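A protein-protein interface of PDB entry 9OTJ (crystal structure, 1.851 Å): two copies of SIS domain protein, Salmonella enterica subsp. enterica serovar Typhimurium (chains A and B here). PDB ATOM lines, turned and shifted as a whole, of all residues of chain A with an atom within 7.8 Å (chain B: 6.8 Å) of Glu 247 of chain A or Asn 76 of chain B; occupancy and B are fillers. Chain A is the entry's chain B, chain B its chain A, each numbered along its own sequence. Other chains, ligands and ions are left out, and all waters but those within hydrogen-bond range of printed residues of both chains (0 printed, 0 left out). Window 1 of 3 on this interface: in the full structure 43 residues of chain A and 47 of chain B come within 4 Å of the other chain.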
ATOM      1  N   ALA A 216      12.114  23.954 -21.160  1.00  0.00           N
ATOM      2  CA  ALA A 216      11.770  24.241 -19.778  1.00  0.00           C
ATOM      3  C   ALA A 216      10.386  23.688 -19.452  1.00  0.00           C
ATOM      4  O   ALA A 216       9.704  23.118 -20.312  1.00  0.00           O
ATOM      5  CB  ALA A 216      11.813  25.730 -19.542  1.00  0.00           C
ATOM      6  N   SER A 217       9.983  23.881 -18.191  1.00  0.00           N
ATOM      7  CA  SER A 217       8.707  23.406 -17.694  1.00  0.00           C
ATOM      8  C   SER A 217       8.410  24.132 -16.388  1.00  0.00           C
ATOM      9  O   SER A 217       9.312  24.744 -15.811  1.00  0.00           O
ATOM     10  CB  SER A 217       8.741  21.925 -17.444  1.00  0.00           C
ATOM     11  OG  SER A 217       9.657  21.619 -16.384  1.00  0.00           O
ATOM     12  N   CYS A 242       9.721  27.030 -28.320  1.00  0.00           N
ATOM     13  CA  CYS A 242       9.980  26.774 -26.913  1.00  0.00           C
ATOM     14  C   CYS A 242       9.303  25.447 -26.548  1.00  0.00           C
ATOM     15  O   CYS A 242       8.101  25.284 -26.766  1.00  0.00           O
ATOM     16  CB  CYS A 242       9.472  27.935 -26.060  1.00  0.00           C
ATOM     17  SG  CYS A 242       9.765  27.728 -24.279  1.00  0.00           S
ATOM     18  N   ILE A 243      10.074  24.499 -25.994  1.00  0.00           N
ATOM     19  CA  ILE A 243       9.623  23.124 -25.846  1.00  0.00           C
ATOM     20  C   ILE A 243       9.363  22.806 -24.367  1.00  0.00           C
ATOM     21  O   ILE A 243      10.292  22.681 -23.577  1.00  0.00           O
ATOM     22  CB  ILE A 243      10.660  22.172 -26.484  1.00  0.00           C
ATOM     23  CG1 ILE A 243      11.088  22.648 -27.891  1.00  0.00           C
ATOM     24  CG2 ILE A 243      10.160  20.719 -26.504  1.00  0.00           C
ATOM     25  CD1 ILE A 243      12.485  22.205 -28.282  1.00  0.00           C
ATOM     26  N   HIS A 244       8.083  22.637 -24.006  1.00  0.00           N
ATOM     27  CA  HIS A 244       7.688  22.125 -22.702  1.00  0.00           C
ATOM     28  C   HIS A 244       8.325  20.746 -22.566  1.00  0.00           C
ATOM     29  O   HIS A 244       8.125  19.894 -23.425  1.00  0.00           O
ATOM     30  CB  HIS A 244       6.159  22.070 -22.535  1.00  0.00           C
ATOM     31  CG  HIS A 244       5.425  23.354 -22.231  1.00  0.00           C
ATOM     32  ND1 HIS A 244       5.579  24.109 -21.085  1.00  0.00           N
ATOM     33  CD2 HIS A 244       4.427  23.949 -22.920  1.00  0.00           C
ATOM     34  CE1 HIS A 244       4.738  25.141 -21.117  1.00  0.00           C
ATOM     35  NE2 HIS A 244       4.035  25.068 -22.226  1.00  0.00           N
ATOM     36  N   SER A 245       9.143  20.592 -21.513  1.00  0.00           N
ATOM     37  CA  SER A 245       9.930  19.398 -21.239  1.00  0.00           C
ATOM     38  C   SER A 245       9.068  18.132 -21.334  1.00  0.00           C
ATOM     39  O   SER A 245       9.535  17.109 -21.852  1.00  0.00           O
ATOM     40  CB  SER A 245      10.591  19.490 -19.870  1.00  0.00           C
ATOM     41  OG  SER A 245      11.584  20.500 -19.808  1.00  0.00           O
ATOM     42  N   GLY A 246       7.828  18.206 -20.804  1.00  0.00           N
ATOM     43  CA  GLY A 246       6.908  17.077 -20.801  1.00  0.00           C
ATOM     44  C   GLY A 246       6.699  16.533 -22.212  1.00  0.00           C
ATOM     45  O   GLY A 246       6.654  15.322 -22.407  1.00  0.00           O
ATOM     46  N   GLU A 247       6.644  17.444 -23.195  1.00  0.00           N
ATOM     47  CA  GLU A 247       6.166  17.137 -24.536  1.00  0.00           C
ATOM     48  C   GLU A 247       7.345  16.743 -25.431  1.00  0.00           C
ATOM     49  O   GLU A 247       7.689  17.465 -26.368  1.00  0.00           O
ATOM     50  CB  GLU A 247       5.320  18.332 -25.005  1.00  0.00           C
ATOM     51  CG  GLU A 247       4.029  18.577 -24.209  1.00  0.00           C
ATOM     52  CD  GLU A 247       2.707  17.958 -24.685  1.00  0.00           C
ATOM     53  OE1 GLU A 247       2.210  16.974 -24.084  1.00  0.00           O
ATOM     54  OE2 GLU A 247       2.112  18.499 -25.645  1.00  0.00           O
ATOM     55  N   PHE A 248       7.971  15.601 -25.105  1.00  0.00           N
ATOM     56  CA  PHE A 248       9.000  14.953 -25.923  1.00  0.00           C
ATOM     57  C   PHE A 248       8.673  13.464 -26.101  1.00  0.00           C
ATOM     58  O   PHE A 248       9.027  12.828 -27.103  1.00  0.00           O
ATOM     59  CB  PHE A 248      10.394  15.046 -25.277  1.00  0.00           C
ATOM     60  CG  PHE A 248      11.288  16.219 -25.665  1.00  0.00           C
ATOM     61  CD1 PHE A 248      11.472  16.582 -26.997  1.00  0.00           C
ATOM     62  CD2 PHE A 248      11.956  16.956 -24.689  1.00  0.00           C
ATOM     63  CE1 PHE A 248      12.292  17.647 -27.339  1.00  0.00           C
ATOM     64  CE2 PHE A 248      12.774  18.022 -25.039  1.00  0.00           C
ATOM     65  CZ  PHE A 248      12.934  18.369 -26.358  1.00  0.00           C
ATOM     66  N   PHE A 249       7.993  12.919 -25.087  1.00  0.00           N
ATOM     67  CA  PHE A 249       7.651  11.510 -25.007  1.00  0.00           C
ATOM     68  C   PHE A 249       6.234  11.352 -25.547  1.00  0.00           C
ATOM     69  O   PHE A 249       5.606  10.314 -25.349  1.00  0.00           O
ATOM     70  CB  PHE A 249       7.831  11.082 -23.545  1.00  0.00           C
ATOM     71  CG  PHE A 249       9.017  11.774 -22.890  1.00  0.00           C
ATOM     72  CD1 PHE A 249       8.868  13.024 -22.293  1.00  0.00           C
ATOM     73  CD2 PHE A 249      10.287  11.206 -22.933  1.00  0.00           C
ATOM     74  CE1 PHE A 249       9.951  13.682 -21.741  1.00  0.00           C
ATOM     75  CE2 PHE A 249      11.364  11.862 -22.359  1.00  0.00           C
ATOM     76  CZ  PHE A 249      11.193  13.099 -21.766  1.00  0.00           C
ATOM     77  N   HIS A 250       5.757  12.419 -26.206  1.00  0.00           N
ATOM     78  CA  HIS A 250       4.449  12.477 -26.834  1.00  0.00           C
ATOM     79  C   HIS A 250       4.666  12.933 -28.277  1.00  0.00           C
ATOM     80  O   HIS A 250       3.863  13.696 -28.808  1.00  0.00           O
ATOM     81  CB  HIS A 250       3.540  13.383 -25.989  1.00  0.00           C
ATOM     82  CG  HIS A 250       3.625  13.103 -24.513  1.00  0.00           C
ATOM     83  ND1 HIS A 250       3.874  14.088 -23.578  1.00  0.00           N
ATOM     84  CD2 HIS A 250       3.531  11.958 -23.806  1.00  0.00           C
ATOM     85  CE1 HIS A 250       3.910  13.551 -22.362  1.00  0.00           C
ATOM     86  NE2 HIS A 250       3.704  12.257 -22.477  1.00  0.00           N
ATOM     87  N   GLY A 251       5.760  12.427 -28.884  1.00  0.00           N
ATOM     88  CA  GLY A 251       6.338  12.817 -30.168  1.00  0.00           C
ATOM     89  C   GLY A 251       5.354  13.410 -31.181  1.00  0.00           C
ATOM     90  O   GLY A 251       4.172  13.066 -31.170  1.00  0.00           O
ATOM     91  N   PRO A 252       5.801  14.248 -32.157  1.00  0.00           N
ATOM     92  CA  PRO A 252       7.205  14.357 -32.548  1.00  0.00           C
ATOM     93  C   PRO A 252       8.131  15.104 -31.583  1.00  0.00           C
ATOM     94  O   PRO A 252       7.699  15.864 -30.720  1.00  0.00           O
ATOM     95  CB  PRO A 252       7.135  15.069 -33.904  1.00  0.00           C
ATOM     96  CG  PRO A 252       5.913  15.944 -33.756  1.00  0.00           C
ATOM     97  CD  PRO A 252       4.933  15.119 -32.969  1.00  0.00           C
ATOM     98  N   PHE A 253       9.430  14.844 -31.761  1.00  0.00           N
ATOM     99  CA  PHE A 253      10.493  15.459 -30.988  1.00  0.00           C
ATOM    100  C   PHE A 253      11.491  16.078 -31.961  1.00  0.00           C
ATOM    101  O   PHE A 253      11.811  15.476 -32.989  1.00  0.00           O
ATOM    102  CB  PHE A 253      11.118  14.434 -30.037  1.00  0.00           C
ATOM    103  CG  PHE A 253      11.182  12.973 -30.483  1.00  0.00           C
ATOM    104  CD1 PHE A 253      12.308  12.474 -31.143  1.00  0.00           C
ATOM    105  CD2 PHE A 253      10.150  12.085 -30.168  1.00  0.00           C
ATOM    106  CE1 PHE A 253      12.387  11.131 -31.491  1.00  0.00           C
ATOM    107  CE2 PHE A 253      10.233  10.749 -30.524  1.00  0.00           C
ATOM    108  CZ  PHE A 253      11.350  10.274 -31.185  1.00  0.00           C
ATOM    109  N   GLU A 254      11.978  17.277 -31.607  1.00  0.00           N
ATOM    110  CA  GLU A 254      12.630  18.174 -32.551  1.00  0.00           C
ATOM    111  C   GLU A 254      14.052  17.687 -32.825  1.00  0.00           C
ATOM    112  O   GLU A 254      15.016  18.385 -32.531  1.00  0.00           O
ATOM    113  CB  GLU A 254      12.605  19.626 -32.060  1.00  0.00           C
ATOM    114  CG  GLU A 254      11.221  20.278 -32.103  1.00  0.00           C
ATOM    115  CD  GLU A 254      10.296  19.972 -30.930  1.00  0.00           C
ATOM    116  OE1 GLU A 254      10.736  19.290 -29.968  1.00  0.00           O
ATOM    117  OE2 GLU A 254       9.126  20.421 -30.967  1.00  0.00           O
ATOM    118  N   VAL A 274      10.465  16.400 -14.176  1.00  0.00           N
ATOM    119  CA  VAL A 274      10.084  16.480 -15.579  1.00  0.00           C
ATOM    120  C   VAL A 274      11.289  16.902 -16.428  1.00  0.00           C
ATOM    121  O   VAL A 274      11.537  16.356 -17.497  1.00  0.00           O
ATOM    122  CB  VAL A 274       8.894  17.451 -15.761  1.00  0.00           C
ATOM    123  CG1 VAL A 274       8.646  17.772 -17.219  1.00  0.00           C
ATOM    124  CG2 VAL A 274       7.602  16.955 -15.102  1.00  0.00           C
ATOM    125  N   ARG A 277      13.952  14.164 -16.916  1.00  0.00           N
ATOM    126  CA  ARG A 277      13.554  13.106 -17.815  1.00  0.00           C
ATOM    127  C   ARG A 277      13.742  13.588 -19.249  1.00  0.00           C
ATOM    128  O   ARG A 277      14.130  12.828 -20.135  1.00  0.00           O
ATOM    129  CB  ARG A 277      12.133  12.700 -17.417  1.00  0.00           C
ATOM    130  CG  ARG A 277      11.625  11.489 -18.181  1.00  0.00           C
ATOM    131  CD  ARG A 277      10.113  11.458 -18.245  1.00  0.00           C
ATOM    132  NE  ARG A 277       9.672  10.620 -19.364  1.00  0.00           N
ATOM    133  CZ  ARG A 277       8.420  10.326 -19.612  1.00  0.00           C
ATOM    134  NH1 ARG A 277       7.445  11.004 -19.057  1.00  0.00           N
ATOM    135  NH2 ARG A 277       8.127   9.349 -20.430  1.00  0.00           N
ATOM    136  N   ALA A 278      13.461  14.869 -19.485  1.00  0.00           N
ATOM    137  CA  ALA A 278      13.737  15.473 -20.775  1.00  0.00           C
ATOM    138  C   ALA A 278      15.242  15.500 -21.086  1.00  0.00           C
ATOM    139  O   ALA A 278      15.643  15.350 -22.241  1.00  0.00           O
ATOM    140  CB  ALA A 278      13.108  16.857 -20.840  1.00  0.00           C
ATOM    141  N   PHE A 281      16.523  12.069 -22.063  1.00  0.00           N
ATOM    142  CA  PHE A 281      16.097  11.822 -23.427  1.00  0.00           C
ATOM    143  C   PHE A 281      17.052  12.416 -24.456  1.00  0.00           C
ATOM    144  O   PHE A 281      17.484  11.690 -25.335  1.00  0.00           O
ATOM    145  CB  PHE A 281      14.685  12.397 -23.568  1.00  0.00           C
ATOM    146  CG  PHE A 281      14.098  12.337 -24.967  1.00  0.00           C
ATOM    147  CD1 PHE A 281      13.454  11.197 -25.424  1.00  0.00           C
ATOM    148  CD2 PHE A 281      14.171  13.434 -25.807  1.00  0.00           C
ATOM    149  CE1 PHE A 281      12.889  11.163 -26.685  1.00  0.00           C
ATOM    150  CE2 PHE A 281      13.626  13.385 -27.075  1.00  0.00           C
ATOM    151  CZ  PHE A 281      12.959  12.264 -27.498  1.00  0.00           C
ATOM    152  N   TYR B  46      -8.486  20.049 -17.165  1.00  0.00           N
ATOM    153  CA  TYR B  46      -8.234  19.295 -18.375  1.00  0.00           C
ATOM    154  C   TYR B  46      -6.779  18.906 -18.341  1.00  0.00           C
ATOM    155  O   TYR B  46      -5.911  19.760 -18.199  1.00  0.00           O
ATOM    156  CB  TYR B  46      -8.668  20.097 -19.604  1.00  0.00           C
ATOM    157  CG  TYR B  46     -10.168  20.339 -19.612  1.00  0.00           C
ATOM    158  CD1 TYR B  46     -11.014  19.388 -20.152  1.00  0.00           C
ATOM    159  CD2 TYR B  46     -10.721  21.477 -19.055  1.00  0.00           C
ATOM    160  CE1 TYR B  46     -12.378  19.564 -20.125  1.00  0.00           C
ATOM    161  CE2 TYR B  46     -12.083  21.677 -19.000  1.00  0.00           C
ATOM    162  CZ  TYR B  46     -12.905  20.697 -19.536  1.00  0.00           C
ATOM    163  OH  TYR B  46     -14.229  20.795 -19.516  1.00  0.00           O
ATOM    164  N   VAL B  47      -6.538  17.596 -18.388  1.00  0.00           N
ATOM    165  CA  VAL B  47      -5.193  17.042 -18.296  1.00  0.00           C
ATOM    166  C   VAL B  47      -4.997  16.014 -19.394  1.00  0.00           C
ATOM    167  O   VAL B  47      -5.750  15.041 -19.518  1.00  0.00           O
ATOM    168  CB  VAL B  47      -4.994  16.408 -16.920  1.00  0.00           C
ATOM    169  CG1 VAL B  47      -3.549  15.969 -16.683  1.00  0.00           C
ATOM    170  CG2 VAL B  47      -5.462  17.369 -15.836  1.00  0.00           C
ATOM    171  N   ALA B  48      -3.943  16.203 -20.150  1.00  0.00           N
ATOM    172  CA  ALA B  48      -3.602  15.316 -21.244  1.00  0.00           C
ATOM    173  C   ALA B  48      -2.170  15.611 -21.682  1.00  0.00           C
ATOM    174  O   ALA B  48      -1.554  16.567 -21.230  1.00  0.00           O
ATOM    175  CB  ALA B  48      -4.531  15.513 -22.437  1.00  0.00           C
ATOM    176  N   CYS B  49      -1.686  14.774 -22.582  1.00  0.00           N
ATOM    177  CA  CYS B  49      -0.482  15.018 -23.352  1.00  0.00           C
ATOM    178  C   CYS B  49      -0.809  15.072 -24.841  1.00  0.00           C
ATOM    179  O   CYS B  49      -1.936  14.782 -25.298  1.00  0.00           O
ATOM    180  CB  CYS B  49       0.502  13.864 -23.199  1.00  0.00           C
ATOM    181  SG  CYS B  49       0.838  13.447 -21.471  1.00  0.00           S
ATOM    182  N   GLY B  50       0.219  15.457 -25.592  1.00  0.00           N
ATOM    183  CA  GLY B  50       0.173  15.365 -27.037  1.00  0.00           C
ATOM    184  C   GLY B  50      -1.023  16.130 -27.585  1.00  0.00           C
ATOM    185  O   GLY B  50      -1.403  17.165 -27.033  1.00  0.00           O
ATOM    186  N   GLY B  51      -1.626  15.539 -28.620  1.00  0.00           N
ATOM    187  CA  GLY B  51      -2.680  16.159 -29.395  1.00  0.00           C
ATOM    188  C   GLY B  51      -3.934  16.321 -28.550  1.00  0.00           C
ATOM    189  O   GLY B  51      -4.724  17.214 -28.785  1.00  0.00           O
ATOM    190  N   TYR B  53      -3.936  17.344 -25.560  1.00  0.00           N
ATOM    191  CA  TYR B  53      -3.727  18.549 -24.783  1.00  0.00           C
ATOM    192  C   TYR B  53      -4.220  19.733 -25.602  1.00  0.00           C
ATOM    193  O   TYR B  53      -5.044  20.531 -25.156  1.00  0.00           O
ATOM    194  CB  TYR B  53      -2.258  18.698 -24.377  1.00  0.00           C
ATOM    195  CG  TYR B  53      -1.908  20.027 -23.745  1.00  0.00           C
ATOM    196  CD1 TYR B  53      -1.523  21.109 -24.529  1.00  0.00           C
ATOM    197  CD2 TYR B  53      -1.981  20.204 -22.371  1.00  0.00           C
ATOM    198  CE1 TYR B  53      -1.178  22.327 -23.965  1.00  0.00           C
ATOM    199  CE2 TYR B  53      -1.618  21.413 -21.787  1.00  0.00           C
ATOM    200  CZ  TYR B  53      -1.225  22.472 -22.589  1.00  0.00           C
ATOM    201  OH  TYR B  53      -0.898  23.659 -22.011  1.00  0.00           O
ATOM    202  N   ALA B  54      -3.792  19.797 -26.846  1.00  0.00           N
ATOM    203  CA  ALA B  54      -4.253  20.881 -27.711  1.00  0.00           C
ATOM    204  C   ALA B  54      -5.769  20.843 -27.896  1.00  0.00           C
ATOM    205  O   ALA B  54      -6.442  21.870 -28.057  1.00  0.00           O
ATOM    206  CB  ALA B  54      -3.528  20.779 -29.024  1.00  0.00           C
ATOM    207  N   LEU B  74      -5.729  23.946 -17.523  1.00  0.00           N
ATOM    208  CA  LEU B  74      -5.327  23.057 -18.611  1.00  0.00           C
ATOM    209  C   LEU B  74      -3.893  22.650 -18.354  1.00  0.00           C
ATOM    210  O   LEU B  74      -3.044  23.520 -18.264  1.00  0.00           O
ATOM    211  CB  LEU B  74      -5.497  23.703 -19.979  1.00  0.00           C
ATOM    212  CG  LEU B  74      -4.936  22.931 -21.183  1.00  0.00           C
ATOM    213  CD1 LEU B  74      -5.475  21.549 -21.252  1.00  0.00           C
ATOM    214  CD2 LEU B  74      -5.274  23.655 -22.448  1.00  0.00           C
ATOM    215  N   TYR B  75      -3.660  21.338 -18.179  1.00  0.00           N
ATOM    216  CA  TYR B  75      -2.390  20.819 -17.733  1.00  0.00           C
ATOM    217  C   TYR B  75      -1.932  19.698 -18.647  1.00  0.00           C
ATOM    218  O   TYR B  75      -2.682  18.818 -19.063  1.00  0.00           O
ATOM    219  CB  TYR B  75      -2.410  20.188 -16.346  1.00  0.00           C
ATOM    220  CG  TYR B  75      -2.474  21.105 -15.138  1.00  0.00           C
ATOM    221  CD1 TYR B  75      -3.666  21.713 -14.740  1.00  0.00           C
ATOM    222  CD2 TYR B  75      -1.347  21.330 -14.356  1.00  0.00           C
ATOM    223  CE1 TYR B  75      -3.744  22.496 -13.612  1.00  0.00           C
ATOM    224  CE2 TYR B  75      -1.405  22.111 -13.212  1.00  0.00           C
ATOM    225  CZ  TYR B  75      -2.604  22.691 -12.834  1.00  0.00           C
ATOM    226  OH  TYR B  75      -2.638  23.439 -11.705  1.00  0.00           O
ATOM    227  N   ASN B  76      -0.645  19.779 -18.955  1.00  0.00           N
ATOM    228  CA  ASN B  76       0.152  18.669 -19.435  1.00  0.00           C
ATOM    229  C   ASN B  76       0.194  17.632 -18.315  1.00  0.00           C
ATOM    230  O   ASN B  76       0.331  18.013 -17.156  1.00  0.00           O
ATOM    231  CB  ASN B  76       1.521  19.210 -19.846  1.00  0.00           C
ATOM    232  CG  ASN B  76       2.563  18.138 -19.741  1.00  0.00           C
ATOM    233  OD1 ASN B  76       3.000  17.842 -18.626  1.00  0.00           O
ATOM    234  ND2 ASN B  76       2.917  17.526 -20.861  1.00  0.00           N
ATOM    235  N   SER B  77       0.064  16.345 -18.658  1.00  0.00           N
ATOM    236  CA  SER B  77      -0.068  15.259 -17.688  1.00  0.00           C
ATOM    237  C   SER B  77       1.107  15.220 -16.703  1.00  0.00           C
ATOM    238  O   SER B  77       0.919  15.120 -15.470  1.00  0.00           O
ATOM    239  CB  SER B  77      -0.259  13.936 -18.390  1.00  0.00           C
ATOM    240  OG  SER B  77      -1.518  13.858 -19.064  1.00  0.00           O
ATOM    241  N   GLY B  78       2.307  15.426 -17.242  1.00  0.00           N
ATOM    242  CA  GLY B  78       3.537  15.386 -16.463  1.00  0.00           C
ATOM    243  C   GLY B  78       3.611  16.503 -15.425  1.00  0.00           C
ATOM    244  O   GLY B  78       3.989  16.272 -14.283  1.00  0.00           O
ATOM    245  N   GLU B  79       3.177  17.704 -15.829  1.00  0.00           N
ATOM    246  CA  GLU B  79       3.096  18.859 -14.964  1.00  0.00           C
ATOM    247  C   GLU B  79       2.134  18.538 -13.837  1.00  0.00           C
ATOM    248  O   GLU B  79       2.449  18.720 -12.659  1.00  0.00           O
ATOM    249  CB  GLU B  79       2.627  20.066 -15.778  1.00  0.00           C
ATOM    250  CG  GLU B  79       3.692  20.725 -16.648  1.00  0.00           C
ATOM    251  CD  GLU B  79       4.458  21.798 -15.890  1.00  0.00           C
ATOM    252  OE1 GLU B  79       3.828  22.826 -15.542  1.00  0.00           O
ATOM    253  OE2 GLU B  79       5.665  21.588 -15.628  1.00  0.00           O
ATOM    254  N   PHE B  80       0.977  17.993 -14.239  1.00  0.00           N
ATOM    255  CA  PHE B  80      -0.109  17.742 -13.322  1.00  0.00           C
ATOM    256  C   PHE B  80       0.330  16.804 -12.199  1.00  0.00           C
ATOM    257  O   PHE B  80       0.080  17.097 -11.026  1.00  0.00           O
ATOM    258  CB  PHE B  80      -1.303  17.133 -14.056  1.00  0.00           C
ATOM    259  CG  PHE B  80      -2.528  17.036 -13.176  1.00  0.00           C
ATOM    260  CD1 PHE B  80      -3.246  18.180 -12.860  1.00  0.00           C
ATOM    261  CD2 PHE B  80      -2.959  15.823 -12.669  1.00  0.00           C
ATOM    262  CE1 PHE B  80      -4.374  18.117 -12.099  1.00  0.00           C
ATOM    263  CE2 PHE B  80      -4.110  15.752 -11.925  1.00  0.00           C
ATOM    264  CZ  PHE B  80      -4.820  16.895 -11.627  1.00  0.00           C
ATOM    265  N   ILE B  81       0.950  15.684 -12.571  1.00  0.00           N
ATOM    266  CA  ILE B  81       1.230  14.631 -11.606  1.00  0.00           C
ATOM    267  C   ILE B  81       2.408  14.988 -10.705  1.00  0.00           C
ATOM    268  O   ILE B  81       2.427  14.570  -9.566  1.00  0.00           O
ATOM    269  CB  ILE B  81       1.442  13.260 -12.275  1.00  0.00           C
ATOM    270  CG1 ILE B  81       2.690  13.179 -13.097  1.00  0.00           C
ATOM    271  CG2 ILE B  81       0.227  12.826 -13.080  1.00  0.00           C
ATOM    272  CD1 ILE B  81       2.914  11.797 -13.670  1.00  0.00           C
ATOM    273  N   GLU B 105       1.320   8.819 -18.017  1.00  0.00           N
ATOM    274  CA  GLU B 105       1.239  10.031 -17.222  1.00  0.00           C
ATOM    275  C   GLU B 105      -0.236  10.362 -17.008  1.00  0.00           C
ATOM    276  O   GLU B 105      -0.627  10.718 -15.897  1.00  0.00           O
ATOM    277  CB  GLU B 105       2.024  11.213 -17.806  1.00  0.00           C
ATOM    278  CG  GLU B 105       3.523  10.960 -18.007  1.00  0.00           C
ATOM    279  CD  GLU B 105       3.838  10.583 -19.443  1.00  0.00           C
ATOM    280  OE1 GLU B 105       3.322   9.544 -19.937  1.00  0.00           O
ATOM    281  OE2 GLU B 105       4.549  11.386 -20.095  1.00  0.00           O
ATOM    282  N   TYR B 225      -1.911  25.218 -33.394  1.00  0.00           N
ATOM    283  CA  TYR B 225      -0.775  24.623 -32.722  1.00  0.00           C
ATOM    284  C   TYR B 225      -0.552  23.220 -33.273  1.00  0.00           C
ATOM    285  O   TYR B 225       0.566  22.887 -33.642  1.00  0.00           O
ATOM    286  CB  TYR B 225      -0.896  24.590 -31.199  1.00  0.00           C
ATOM    287  CG  TYR B 225       0.295  23.912 -30.538  1.00  0.00           C
ATOM    288  CD1 TYR B 225       1.530  24.547 -30.506  1.00  0.00           C
ATOM    289  CD2 TYR B 225       0.199  22.648 -29.947  1.00  0.00           C
ATOM    290  CE1 TYR B 225       2.635  23.963 -29.903  1.00  0.00           C
ATOM    291  CE2 TYR B 225       1.293  22.053 -29.326  1.00  0.00           C
ATOM    292  CZ  TYR B 225       2.513  22.716 -29.313  1.00  0.00           C
ATOM    293  OH  TYR B 225       3.641  22.211 -28.750  1.00  0.00           O
ATOM    294  N   ILE B 229       2.581  21.310 -35.883  1.00  0.00           N
ATOM    295  CA  ILE B 229       3.170  20.001 -35.637  1.00  0.00           C
ATOM    296  C   ILE B 229       3.023  19.098 -36.858  1.00  0.00           C
ATOM    297  O   ILE B 229       3.996  18.443 -37.215  1.00  0.00           O
ATOM    298  CB  ILE B 229       2.561  19.365 -34.379  1.00  0.00           C
ATOM    299  CG1 ILE B 229       3.150  20.058 -33.149  1.00  0.00           C
ATOM    300  CG2 ILE B 229       2.749  17.845 -34.340  1.00  0.00           C
ATOM    301  CD1 ILE B 229       2.519  19.657 -31.833  1.00  0.00           C
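NE2 of His 250 of chain A sits at hydrogen-bond distance from OE2 of Glu 105 of chain B, 2.7 Å away.
OE2 of Glu 105 of chain B is in salt-bridge range of NH1 of Arg 277 of chain A.
N of Gly 50 of chain B sits at hydrogen-bond distance from OE1 of Glu 247 of chain A (2.9 Å).
The side-chain carboxylate of Glu 247 of chain A is in hydrogen-bond range of the side-chain amide nitrogen of Asn 76 of chain B (3.3 Å).
NE2 of His 250 of chain A sits close to SG of Cys 49 of chain B, 3.3 Å away.
The backbone NH of Gly 78 of chain B lies within hydrogen-bond range of the side-chain amide oxygen of Asn 76 of chain B (2.9 Å).
ND1 of His 250 of chain A sits at hydrogen-bond distance from O of Gly 246 of chain A.
SG of Cys 49 of chain B lies close to OG of Ser 77 of chain B (3.4 Å).
OE1 of Glu 247 of chain A sits at hydrogen-bond distance from ND1 of His 250 of chain A, 3.4 Å away.
OD1 of Asn 76 of chain B lies within hydrogen-bond range of N of Glu 79 of chain B (2.8 Å).
Among the printed residues, pairs that only touch across the chains: Ser 217 of chain A with Glu 79 of chain B, Glu 247 of chain A with Cys 49 of chain B, His 250 of chain A with Gly 50 of chain B, Pro 252 of chain A with Ile 229 of chain B and Val 274 of chain A with Gly 78 of chain B.
Of chain B, only Cys 49 (3.4 Å), Gly 50 (2.9 Å) and Asn 76 (3.3 Å) come within 4 Å of Glu 247 of chain A.
Of the printed residues of chain A, Asn 76 of chain B touches Glu 247 (3.3 Å).
Printed residues of chain B within 4 Å of Arg 277 of chain A: Glu 105 (3.1 Å).
Printed residues of chain A within 4 Å of Glu 79 of chain B: Ser 217.
Of the printed residues of chain B, Pro 252 of chain A touches Ile 229 (3.7 Å).
Printed residues of chain B within 4 Å of Ser 217 of chain A: Glu 79 (3.6 Å).
Of the printed residues of chain A, Ile 229 of chain B touches Pro 252 (3.7 Å).
Val 47 of chain B touches none of the printed residues of chain A.
Phe 281 of chain A touches none of the printed residues of chain B.
The nearest residue of chain B that does not touch Glu 247 of chain A is Tyr 53 of chain B (4.6 Å).
The nearest printed residue of chain A that does not touch Asn 76 of chain B is Gly 246 of chain A (4.02 Å).
The nearest printed residue of chain A that does not touch Glu 105 of chain B is Phe 249 of chain A (4.8 Å).
Hydrophobic or aromatic side chains of chain A within 4 Å of the printed part of chain B: His 250, Pro 252 and Val 274.
Of the 19 printed residues of chain B, 7 touch a printed residue of chain A.
No position is printed for both chains.
Of the 10 pairs that touch across the chains among the printed residues, none has its exchanged pair printed and touching as well.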
